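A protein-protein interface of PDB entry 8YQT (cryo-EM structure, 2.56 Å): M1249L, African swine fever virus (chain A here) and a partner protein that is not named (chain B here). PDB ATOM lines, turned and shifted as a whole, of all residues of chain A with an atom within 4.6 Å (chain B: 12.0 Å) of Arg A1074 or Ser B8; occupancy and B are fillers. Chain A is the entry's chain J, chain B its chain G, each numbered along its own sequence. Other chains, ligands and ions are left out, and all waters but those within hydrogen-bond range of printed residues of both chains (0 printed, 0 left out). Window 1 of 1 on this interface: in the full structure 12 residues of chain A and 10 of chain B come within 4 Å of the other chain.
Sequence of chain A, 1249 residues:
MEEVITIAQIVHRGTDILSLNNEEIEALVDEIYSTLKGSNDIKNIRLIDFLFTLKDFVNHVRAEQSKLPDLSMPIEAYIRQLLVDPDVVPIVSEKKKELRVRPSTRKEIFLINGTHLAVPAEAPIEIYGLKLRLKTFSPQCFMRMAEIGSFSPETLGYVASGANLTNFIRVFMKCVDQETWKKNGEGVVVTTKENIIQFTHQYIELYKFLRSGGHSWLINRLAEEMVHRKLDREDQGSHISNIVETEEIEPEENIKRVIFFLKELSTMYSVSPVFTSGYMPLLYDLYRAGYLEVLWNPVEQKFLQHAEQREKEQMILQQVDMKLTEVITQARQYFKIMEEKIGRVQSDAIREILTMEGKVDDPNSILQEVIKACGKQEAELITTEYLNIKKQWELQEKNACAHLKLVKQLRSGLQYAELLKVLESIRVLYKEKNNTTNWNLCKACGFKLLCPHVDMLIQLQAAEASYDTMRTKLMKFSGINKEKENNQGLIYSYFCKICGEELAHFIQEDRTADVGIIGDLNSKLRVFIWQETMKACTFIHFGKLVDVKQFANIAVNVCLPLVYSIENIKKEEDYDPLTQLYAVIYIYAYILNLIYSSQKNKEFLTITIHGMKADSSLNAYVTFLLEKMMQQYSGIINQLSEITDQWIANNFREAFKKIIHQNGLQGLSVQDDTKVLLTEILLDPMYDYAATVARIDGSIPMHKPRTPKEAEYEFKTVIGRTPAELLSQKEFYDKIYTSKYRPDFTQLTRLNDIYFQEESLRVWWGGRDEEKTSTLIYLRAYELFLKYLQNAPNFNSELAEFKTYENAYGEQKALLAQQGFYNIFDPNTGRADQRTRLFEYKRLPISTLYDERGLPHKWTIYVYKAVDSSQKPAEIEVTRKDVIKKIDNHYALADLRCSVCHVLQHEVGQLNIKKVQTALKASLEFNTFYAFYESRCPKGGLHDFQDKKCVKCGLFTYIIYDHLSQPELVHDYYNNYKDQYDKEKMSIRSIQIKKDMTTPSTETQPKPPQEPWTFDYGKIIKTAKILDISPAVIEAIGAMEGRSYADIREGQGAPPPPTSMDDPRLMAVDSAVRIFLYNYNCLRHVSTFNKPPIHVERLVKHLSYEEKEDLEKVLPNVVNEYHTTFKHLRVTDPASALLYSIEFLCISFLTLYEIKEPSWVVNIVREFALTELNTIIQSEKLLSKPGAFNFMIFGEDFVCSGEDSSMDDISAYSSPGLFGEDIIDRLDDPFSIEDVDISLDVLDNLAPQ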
ATOM      1  N   ASP A1070      -8.747   3.784 -33.028  1.00  0.00           N
ATOM      2  CA  ASP A1070      -8.304   2.512 -32.467  1.00  0.00           C
ATOM      3  C   ASP A1070      -9.436   1.800 -31.742  1.00  0.00           C
ATOM      4  O   ASP A1070      -9.477   0.565 -31.717  1.00  0.00           O
ATOM      5  CB  ASP A1070      -7.124   2.739 -31.523  1.00  0.00           C
ATOM      6  CG  ASP A1070      -6.607   1.452 -30.915  1.00  0.00           C
ATOM      7  OD1 ASP A1070      -6.020   0.638 -31.655  1.00  0.00           O
ATOM      8  OD2 ASP A1070      -6.777   1.258 -29.693  1.00  0.00           O
ATOM      9  N   SER A1071     -10.359   2.558 -31.147  1.00  0.00           N
ATOM     10  CA  SER A1071     -11.533   1.954 -30.526  1.00  0.00           C
ATOM     11  C   SER A1071     -12.386   1.233 -31.561  1.00  0.00           C
ATOM     12  O   SER A1071     -12.887   0.132 -31.312  1.00  0.00           O
ATOM     13  CB  SER A1071     -12.350   3.026 -29.807  1.00  0.00           C
ATOM     14  OG  SER A1071     -13.583   2.505 -29.349  1.00  0.00           O
ATOM     15  N   ALA A1072     -12.564   1.848 -32.731  1.00  0.00           N
ATOM     16  CA  ALA A1072     -13.364   1.233 -33.784  1.00  0.00           C
ATOM     17  C   ALA A1072     -12.711  -0.040 -34.308  1.00  0.00           C
ATOM     18  O   ALA A1072     -13.404  -1.008 -34.641  1.00  0.00           O
ATOM     19  CB  ALA A1072     -13.583   2.228 -34.920  1.00  0.00           C
ATOM     20  N   VAL A1073     -11.380  -0.055 -34.399  1.00  0.00           N
ATOM     21  CA  VAL A1073     -10.688  -1.219 -34.945  1.00  0.00           C
ATOM     22  C   VAL A1073     -10.908  -2.439 -34.061  1.00  0.00           C
ATOM     23  O   VAL A1073     -11.204  -3.533 -34.553  1.00  0.00           O
ATOM     24  CB  VAL A1073      -9.190  -0.917 -35.130  1.00  0.00           C
ATOM     25  CG1 VAL A1073      -8.445  -2.182 -35.487  1.00  0.00           C
ATOM     26  CG2 VAL A1073      -8.992   0.127 -36.207  1.00  0.00           C
ATOM     27  N   ARG A1074     -10.775  -2.276 -32.745  1.00  0.00           N
ATOM     28  CA  ARG A1074     -10.938  -3.417 -31.856  1.00  0.00           C
ATOM     29  C   ARG A1074     -12.396  -3.809 -31.670  1.00  0.00           C
ATOM     30  O   ARG A1074     -12.668  -4.941 -31.261  1.00  0.00           O
ATOM     31  CB  ARG A1074     -10.293  -3.137 -30.496  1.00  0.00           C
ATOM     32  CG  ARG A1074     -11.132  -2.318 -29.539  1.00  0.00           C
ATOM     33  CD  ARG A1074     -10.393  -2.102 -28.226  1.00  0.00           C
ATOM     34  NE  ARG A1074      -9.216  -1.258 -28.403  1.00  0.00           N
ATOM     35  CZ  ARG A1074      -7.966  -1.693 -28.337  1.00  0.00           C
ATOM     36  NH1 ARG A1074      -7.690  -2.960 -28.081  1.00  0.00           N
ATOM     37  NH2 ARG A1074      -6.970  -0.838 -28.538  1.00  0.00           N
ATOM     38  N   ILE A1075     -13.337  -2.907 -31.956  1.00  0.00           N
ATOM     39  CA  ILE A1075     -14.744  -3.298 -32.012  1.00  0.00           C
ATOM     40  C   ILE A1075     -14.964  -4.278 -33.155  1.00  0.00           C
ATOM     41  O   ILE A1075     -15.670  -5.283 -33.014  1.00  0.00           O
ATOM     42  CB  ILE A1075     -15.645  -2.057 -32.150  1.00  0.00           C
ATOM     43  CG1 ILE A1075     -15.736  -1.307 -30.825  1.00  0.00           C
ATOM     44  CG2 ILE A1075     -17.034  -2.448 -32.604  1.00  0.00           C
ATOM     45  CD1 ILE A1075     -16.251   0.099 -30.974  1.00  0.00           C
ATOM     46  N   PHE A1076     -14.357  -3.995 -34.310  1.00  0.00           N
ATOM     47  CA  PHE A1076     -14.413  -4.928 -35.430  1.00  0.00           C
ATOM     48  C   PHE A1076     -13.723  -6.243 -35.090  1.00  0.00           C
ATOM     49  O   PHE A1076     -14.236  -7.322 -35.405  1.00  0.00           O
ATOM     50  CB  PHE A1076     -13.771  -4.294 -36.663  1.00  0.00           C
ATOM     51  CG  PHE A1076     -13.986  -5.071 -37.926  1.00  0.00           C
ATOM     52  CD1 PHE A1076     -15.129  -4.886 -38.680  1.00  0.00           C
ATOM     53  CD2 PHE A1076     -13.047  -5.991 -38.358  1.00  0.00           C
ATOM     54  CE1 PHE A1076     -15.329  -5.600 -39.843  1.00  0.00           C
ATOM     55  CE2 PHE A1076     -13.242  -6.707 -39.517  1.00  0.00           C
ATOM     56  CZ  PHE A1076     -14.385  -6.510 -40.261  1.00  0.00           C
ATOM     57  N   LEU A1077     -12.556  -6.173 -34.448  1.00  0.00           N
ATOM     58  CA  LEU A1077     -11.783  -7.382 -34.180  1.00  0.00           C
ATOM     59  C   LEU A1077     -12.411  -8.213 -33.068  1.00  0.00           C
ATOM     60  O   LEU A1077     -12.364  -9.447 -33.107  1.00  0.00           O
ATOM     61  CB  LEU A1077     -10.345  -7.009 -33.830  1.00  0.00           C
ATOM     62  CG  LEU A1077      -9.573  -6.352 -34.972  1.00  0.00           C
ATOM     63  CD1 LEU A1077      -8.291  -5.735 -34.457  1.00  0.00           C
ATOM     64  CD2 LEU A1077      -9.287  -7.356 -36.074  1.00  0.00           C
ATOM     65  N   TYR A1078     -12.984  -7.556 -32.059  1.00  0.00           N
ATOM     66  CA  TYR A1078     -13.683  -8.284 -31.004  1.00  0.00           C
ATOM     67  C   TYR A1078     -14.893  -9.020 -31.562  1.00  0.00           C
ATOM     68  O   TYR A1078     -15.128 -10.190 -31.238  1.00  0.00           O
ATOM     69  CB  TYR A1078     -14.105  -7.320 -29.896  1.00  0.00           C
ATOM     70  CG  TYR A1078     -14.859  -7.966 -28.757  1.00  0.00           C
ATOM     71  CD1 TYR A1078     -14.185  -8.540 -27.690  1.00  0.00           C
ATOM     72  CD2 TYR A1078     -16.245  -8.000 -28.751  1.00  0.00           C
ATOM     73  CE1 TYR A1078     -14.871  -9.130 -26.648  1.00  0.00           C
ATOM     74  CE2 TYR A1078     -16.937  -8.590 -27.716  1.00  0.00           C
ATOM     75  CZ  TYR A1078     -16.247  -9.152 -26.668  1.00  0.00           C
ATOM     76  OH  TYR A1078     -16.939  -9.737 -25.634  1.00  0.00           O
ATOM     77  N   HIS A1123      -1.752  -3.986 -33.407  1.00  0.00           N
ATOM     78  CA  HIS A1123      -1.575  -3.341 -32.112  1.00  0.00           C
ATOM     79  C   HIS A1123      -0.139  -2.876 -31.904  1.00  0.00           C
ATOM     80  O   HIS A1123       0.096  -1.813 -31.319  1.00  0.00           O
ATOM     81  CB  HIS A1123      -2.000  -4.292 -30.997  1.00  0.00           C
ATOM     82  CG  HIS A1123      -3.458  -4.625 -31.013  1.00  0.00           C
ATOM     83  ND1 HIS A1123      -4.431  -3.728 -30.630  1.00  0.00           N
ATOM     84  CD2 HIS A1123      -4.110  -5.761 -31.357  1.00  0.00           C
ATOM     85  CE1 HIS A1123      -5.619  -4.295 -30.740  1.00  0.00           C
ATOM     86  NE2 HIS A1123      -5.452  -5.528 -31.180  1.00  0.00           N
ATOM     87  N   MET B   1      -1.061 -10.312 -15.446  1.00  0.00           N
ATOM     88  CA  MET B   1      -2.215 -10.457 -16.322  1.00  0.00           C
ATOM     89  C   MET B   1      -1.797 -10.929 -17.708  1.00  0.00           C
ATOM     90  O   MET B   1      -0.614 -10.942 -18.040  1.00  0.00           O
ATOM     91  CB  MET B   1      -2.972  -9.134 -16.439  1.00  0.00           C
ATOM     92  CG  MET B   1      -2.359  -8.168 -17.435  1.00  0.00           C
ATOM     93  SD  MET B   1      -2.527  -6.447 -16.944  1.00  0.00           S
ATOM     94  CE  MET B   1      -1.577  -5.645 -18.228  1.00  0.00           C
ATOM     95  N   LYS B   2      -2.782 -11.316 -18.513  1.00  0.00           N
ATOM     96  CA  LYS B   2      -2.558 -11.699 -19.900  1.00  0.00           C
ATOM     97  C   LYS B   2      -3.429 -10.827 -20.788  1.00  0.00           C
ATOM     98  O   LYS B   2      -4.596 -10.584 -20.471  1.00  0.00           O
ATOM     99  CB  LYS B   2      -2.870 -13.179 -20.125  1.00  0.00           C
ATOM    100  CG  LYS B   2      -2.688 -13.638 -21.555  1.00  0.00           C
ATOM    101  CD  LYS B   2      -1.226 -13.676 -21.936  1.00  0.00           C
ATOM    102  CE  LYS B   2      -0.845 -15.025 -22.512  1.00  0.00           C
ATOM    103  NZ  LYS B   2       0.631 -15.183 -22.625  1.00  0.00           N
ATOM    104  N   ILE B   3      -2.861 -10.361 -21.896  1.00  0.00           N
ATOM    105  CA  ILE B   3      -3.535  -9.445 -22.809  1.00  0.00           C
ATOM    106  C   ILE B   3      -3.885 -10.194 -24.086  1.00  0.00           C
ATOM    107  O   ILE B   3      -3.015 -10.819 -24.707  1.00  0.00           O
ATOM    108  CB  ILE B   3      -2.657  -8.218 -23.108  1.00  0.00           C
ATOM    109  CG1 ILE B   3      -2.554  -7.325 -21.868  1.00  0.00           C
ATOM    110  CG2 ILE B   3      -3.196  -7.448 -24.296  1.00  0.00           C
ATOM    111  CD1 ILE B   3      -3.890  -6.864 -21.328  1.00  0.00           C
ATOM    112  N   CYS B   4      -5.157 -10.134 -24.477  1.00  0.00           N
ATOM    113  CA  CYS B   4      -5.605 -10.797 -25.694  1.00  0.00           C
ATOM    114  C   CYS B   4      -4.918 -10.201 -26.915  1.00  0.00           C
ATOM    115  O   CYS B   4      -4.709  -8.989 -27.002  1.00  0.00           O
ATOM    116  CB  CYS B   4      -7.123 -10.675 -25.833  1.00  0.00           C
ATOM    117  SG  CYS B   4      -7.813 -11.475 -27.300  1.00  0.00           S
ATOM    118  N   LYS B   5      -4.568 -11.063 -27.866  1.00  0.00           N
ATOM    119  CA  LYS B   5      -3.837 -10.628 -29.047  1.00  0.00           C
ATOM    120  C   LYS B   5      -4.704  -9.887 -30.055  1.00  0.00           C
ATOM    121  O   LYS B   5      -4.158  -9.284 -30.985  1.00  0.00           O
ATOM    122  CB  LYS B   5      -3.180 -11.829 -29.726  1.00  0.00           C
ATOM    123  CG  LYS B   5      -2.002 -12.398 -28.959  1.00  0.00           C
ATOM    124  CD  LYS B   5      -0.934 -11.343 -28.730  1.00  0.00           C
ATOM    125  CE  LYS B   5       0.059 -11.303 -29.877  1.00  0.00           C
ATOM    126  NZ  LYS B   5       0.848 -10.041 -29.880  1.00  0.00           N
ATOM    127  N   ALA B   6      -6.027  -9.908 -29.897  1.00  0.00           N
ATOM    128  CA  ALA B   6      -6.935  -9.277 -30.846  1.00  0.00           C
ATOM    129  C   ALA B   6      -7.666  -8.084 -30.245  1.00  0.00           C
ATOM    130  O   ALA B   6      -7.588  -6.976 -30.785  1.00  0.00           O
ATOM    131  CB  ALA B   6      -7.942 -10.310 -31.372  1.00  0.00           C
ATOM    132  N   CYS B   7      -8.382  -8.275 -29.141  1.00  0.00           N
ATOM    133  CA  CYS B   7      -9.122  -7.195 -28.505  1.00  0.00           C
ATOM    134  C   CYS B   7      -8.344  -6.515 -27.386  1.00  0.00           C
ATOM    135  O   CYS B   7      -8.838  -5.537 -26.817  1.00  0.00           O
ATOM    136  CB  CYS B   7     -10.458  -7.716 -27.967  1.00  0.00           C
ATOM    137  SG  CYS B   7     -10.317  -9.002 -26.710  1.00  0.00           S
ATOM    138  N   SER B   8      -7.148  -7.011 -27.063  1.00  0.00           N
ATOM    139  CA  SER B   8      -6.289  -6.430 -26.028  1.00  0.00           C
ATOM    140  C   SER B   8      -7.007  -6.327 -24.685  1.00  0.00           C
ATOM    141  O   SER B   8      -6.821  -5.368 -23.934  1.00  0.00           O
ATOM    142  CB  SER B   8      -5.747  -5.067 -26.459  1.00  0.00           C
ATOM    143  OG  SER B   8      -4.751  -5.209 -27.456  1.00  0.00           O
ATOM    144  N   SER B   9      -7.828  -7.324 -24.375  1.00  0.00           N
ATOM    145  CA  SER B   9      -8.514  -7.384 -23.096  1.00  0.00           C
ATOM    146  C   SER B   9      -7.690  -8.179 -22.089  1.00  0.00           C
ATOM    147  O   SER B   9      -6.696  -8.823 -22.428  1.00  0.00           O
ATOM    148  CB  SER B   9      -9.900  -8.007 -23.254  1.00  0.00           C
ATOM    149  OG  SER B   9     -10.895  -7.013 -23.419  1.00  0.00           O
ATOM    150  N   CYS B  10      -8.116  -8.126 -20.831  1.00  0.00           N
ATOM    151  CA  CYS B  10      -7.483  -8.890 -19.763  1.00  0.00           C
ATOM    152  C   CYS B  10      -8.163 -10.251 -19.681  1.00  0.00           C
ATOM    153  O   CYS B  10      -9.315 -10.354 -19.252  1.00  0.00           O
ATOM    154  CB  CYS B  10      -7.572  -8.143 -18.435  1.00  0.00           C
ATOM    155  SG  CYS B  10      -6.694  -8.947 -17.082  1.00  0.00           S
ATOM    156  N   MET B  11      -7.451 -11.294 -20.097  1.00  0.00           N
ATOM    157  CA  MET B  11      -8.022 -12.629 -20.164  1.00  0.00           C
ATOM    158  C   MET B  11      -8.107 -13.260 -18.778  1.00  0.00           C
ATOM    159  O   MET B  11      -7.289 -12.988 -17.895  1.00  0.00           O
ATOM    160  CB  MET B  11      -7.190 -13.509 -21.094  1.00  0.00           C
ATOM    161  CG  MET B  11      -7.004 -12.919 -22.480  1.00  0.00           C
ATOM    162  SD  MET B  11      -5.761 -13.776 -23.458  1.00  0.00           S
ATOM    163  CE  MET B  11      -6.678 -15.208 -24.007  1.00  0.00           C
ATOM    164  N   VAL B  12      -9.109 -14.114 -18.596  1.00  0.00           N
ATOM    165  CA  VAL B  12      -9.364 -14.768 -17.317  1.00  0.00           C
ATOM    166  C   VAL B  12      -8.555 -16.057 -17.250  1.00  0.00           C
ATOM    167  O   VAL B  12      -8.456 -16.792 -18.239  1.00  0.00           O
ATOM    168  CB  VAL B  12     -10.864 -15.047 -17.135  1.00  0.00           C
ATOM    169  CG1 VAL B  12     -11.121 -15.758 -15.820  1.00  0.00           C
ATOM    170  CG2 VAL B  12     -11.656 -13.755 -17.211  1.00  0.00           C
ATOM    171  N   PHE B  22      -5.834 -19.200 -20.591  1.00  0.00           N
ATOM    172  CA  PHE B  22      -6.415 -17.868 -20.558  1.00  0.00           C
ATOM    173  C   PHE B  22      -7.568 -17.807 -21.545  1.00  0.00           C
ATOM    174  O   PHE B  22      -7.389 -18.086 -22.735  1.00  0.00           O
ATOM    175  CB  PHE B  22      -5.367 -16.809 -20.888  1.00  0.00           C
ATOM    176  CG  PHE B  22      -4.298 -16.682 -19.852  1.00  0.00           C
ATOM    177  CD1 PHE B  22      -4.519 -15.951 -18.700  1.00  0.00           C
ATOM    178  CD2 PHE B  22      -3.076 -17.305 -20.021  1.00  0.00           C
ATOM    179  CE1 PHE B  22      -3.538 -15.831 -17.745  1.00  0.00           C
ATOM    180  CE2 PHE B  22      -2.094 -17.191 -19.068  1.00  0.00           C
ATOM    181  CZ  PHE B  22      -2.326 -16.453 -17.927  1.00  0.00           C
ATOM    182  N   ARG B  23      -8.747 -17.456 -21.040  1.00  0.00           N
ATOM    183  CA  ARG B  23      -9.967 -17.363 -21.828  1.00  0.00           C
ATOM    184  C   ARG B  23     -10.432 -15.916 -21.827  1.00  0.00           C
ATOM    185  O   ARG B  23     -10.622 -15.323 -20.760  1.00  0.00           O
ATOM    186  CB  ARG B  23     -11.059 -18.272 -21.259  1.00  0.00           C
ATOM    187  CG  ARG B  23     -11.446 -19.441 -22.147  1.00  0.00           C
ATOM    188  CD  ARG B  23     -10.392 -20.532 -22.109  1.00  0.00           C
ATOM    189  NE  ARG B  23     -10.665 -21.594 -23.071  1.00  0.00           N
ATOM    190  CZ  ARG B  23     -10.991 -22.837 -22.744  1.00  0.00           C
ATOM    191  NH1 ARG B  23     -11.096 -23.215 -21.482  1.00  0.00           N
ATOM    192  NH2 ARG B  23     -11.214 -23.723 -23.710  1.00  0.00           N
ATOM    193  N   CYS B  24     -10.616 -15.353 -23.014  1.00  0.00           N
ATOM    194  CA  CYS B  24     -11.149 -14.010 -23.144  1.00  0.00           C
ATOM    195  C   CYS B  24     -12.646 -14.059 -23.435  1.00  0.00           C
ATOM    196  O   CYS B  24     -13.196 -15.083 -23.842  1.00  0.00           O
ATOM    197  CB  CYS B  24     -10.416 -13.246 -24.245  1.00  0.00           C
ATOM    198  SG  CYS B  24     -10.955 -11.535 -24.424  1.00  0.00           S
ATOM    199  N   SER B  25     -13.309 -12.925 -23.222  1.00  0.00           N
ATOM    200  CA  SER B  25     -14.732 -12.813 -23.515  1.00  0.00           C
ATOM    201  C   SER B  25     -15.027 -12.804 -25.009  1.00  0.00           C
ATOM    202  O   SER B  25     -16.198 -12.892 -25.392  1.00  0.00           O
ATOM    203  CB  SER B  25     -15.307 -11.553 -22.861  1.00  0.00           C
ATOM    204  OG  SER B  25     -14.754 -10.381 -23.430  1.00  0.00           O
ATOM    205  N   CYS B  26     -14.005 -12.698 -25.855  1.00  0.00           N
ATOM    206  CA  CYS B  26     -14.168 -12.766 -27.299  1.00  0.00           C
ATOM    207  C   CYS B  26     -14.051 -14.183 -27.840  1.00  0.00           C
ATOM    208  O   CYS B  26     -14.145 -14.377 -29.054  1.00  0.00           O
ATOM    209  CB  CYS B  26     -13.138 -11.871 -27.995  1.00  0.00           C
ATOM    210  SG  CYS B  26     -11.433 -12.455 -27.897  1.00  0.00           S
ATOM    211  N   GLY B  27     -13.844 -15.171 -26.972  1.00  0.00           N
ATOM    212  CA  GLY B  27     -13.695 -16.546 -27.391  1.00  0.00           C
ATOM    213  C   GLY B  27     -12.268 -17.006 -27.582  1.00  0.00           C
ATOM    214  O   GLY B  27     -12.035 -18.216 -27.692  1.00  0.00           O
ATOM    215  N   GLU B  28     -11.308 -16.087 -27.620  1.00  0.00           N
ATOM    216  CA  GLU B  28      -9.911 -16.465 -27.782  1.00  0.00           C
ATOM    217  C   GLU B  28      -9.404 -17.181 -26.537  1.00  0.00           C
ATOM    218  O   GLU B  28      -9.641 -16.736 -25.410  1.00  0.00           O
ATOM    219  CB  GLU B  28      -9.060 -15.231 -28.063  1.00  0.00           C
ATOM    220  CG  GLU B  28      -8.634 -15.085 -29.510  1.00  0.00           C
ATOM    221  CD  GLU B  28      -7.323 -15.781 -29.798  1.00  0.00           C
ATOM    222  OE1 GLU B  28      -7.085 -16.141 -30.970  1.00  0.00           O
ATOM    223  OE2 GLU B  28      -6.529 -15.967 -28.853  1.00  0.00           O
ATOM    224  N   SER B  29      -8.710 -18.294 -26.743  1.00  0.00           N
ATOM    225  CA  SER B  29      -8.099 -19.052 -25.664  1.00  0.00           C
ATOM    226  C   SER B  29      -6.628 -19.277 -25.977  1.00  0.00           C
ATOM    227  O   SER B  29      -6.258 -19.583 -27.114  1.00  0.00           O
ATOM    228  CB  SER B  29      -8.800 -20.398 -25.457  1.00  0.00           C
ATOM    229  OG  SER B  29      -8.618 -21.247 -26.576  1.00  0.00           O
ATOM    230  N   VAL B  30      -5.789 -19.119 -24.955  1.00  0.00           N
ATOM    231  CA  VAL B  30      -4.348 -19.271 -25.107  1.00  0.00           C
ATOM    232  C   VAL B  30      -3.805 -20.089 -23.943  1.00  0.00           C
ATOM    233  O   VAL B  30      -4.450 -20.243 -22.904  1.00  0.00           O
ATOM    234  CB  VAL B  30      -3.627 -17.904 -25.199  1.00  0.00           C
ATOM    235  CG1 VAL B  30      -3.312 -17.367 -23.815  1.00  0.00           C
ATOM    236  CG2 VAL B  30      -2.369 -18.010 -26.044  1.00  0.00           C
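Of the 21 printed residues of chain B, 6 touch a printed residue of chain A. Printed residues of chain A that touch a printed residue of chain B: Arg A1074, Leu A1077, Tyr A1078 and His A1123. Hydrophobic or aromatic side chains of chain A that line the printed part of chain B: Leu A1077, Tyr A1078 and His A1123. Among the printed residues, 9 pairs touch across the chains. Among the printed residues, no Asp or Glu carboxylate lies within 4 Å of a Lys or Arg side-chain nitrogen of the other chain.
Among the printed residues, pairs that only touch across the chains: Arg A1074 with Ser B8 (3.3 Å), Tyr A1078 with Cys B26 (3.5 Å), His A1123 with Ser B8 (3.5 Å), His A1123 with Lys B5 (3.5 Å), Tyr A1078 with Cys B7 (3.8 Å) and Leu A1077 with Ala B6 (3.9 Å).
NE2 of His A1123 sits at hydrogen-bond distance from O of Ala B6 (2.6 Å). The backbone carbonyl oxygen of Cys B7 lies within hydrogen-bond range of the guanidinium group of Arg A1074, at 3.1 Å. OG of Ser B25 is in hydrogen-bond range of OH of Tyr A1078, at 3.2 Å.
SG of Cys B4 sits at hydrogen-bond distance from SG of Cys B7, at 3.6 Å. SG of Cys B4 lies within hydrogen-bond range of SG of Cys B26. The side-chain sulfur of Cys B24 is in hydrogen-bond range of the side-chain sulfur of Cys B7 (3.5 Å). The backbone NH (N) of Cys B26 sits close to the side-chain sulfur (SG) of Cys B24 (3.6 Å). The backbone NH of Glu B28 sits close to the side-chain sulfur of Cys B26 (3.6 Å). OD2 of Asp A1070 lies within salt-bridge range of NH2 of Arg A1074 (2.4 Å).
Of chain B, only Cys B7 and Ser B8 come within 4 Å of Arg A1074. Ser B8 touches two residues of chain A. Asp A1070 touches none of the printed residues of chain B. No residue of chain B comes within 4 Å of Ser A1071. No residue of chain B comes within 4 Å of Ala A1072. No residue of chain B comes within 4 Å of Val A1073. No residue of chain B comes within 4 Å of Ile A1075. Of chain B, only Ala B6 comes within 4 Å of Leu A1077. His A1123 touches three residues of chain B. Of the printed residues of chain A, Lys B5 touches His A1123 (3.5 Å). Printed residues of chain A within 4 Å of Ser B25: Tyr A1078. Of the printed residues of chain A, Cys B26 touches Tyr A1078 (3.5 Å). Met B11 touches none of the printed residues of chain A. Ser B9 touches none of the printed residues of chain A. The nearest printed residue of chain A that does not touch Ser B8 is Asp A1070 (7.1 Å). The nearest printed residue of chain A that does not touch Cys B26 is Leu A1077 (5.7 Å).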
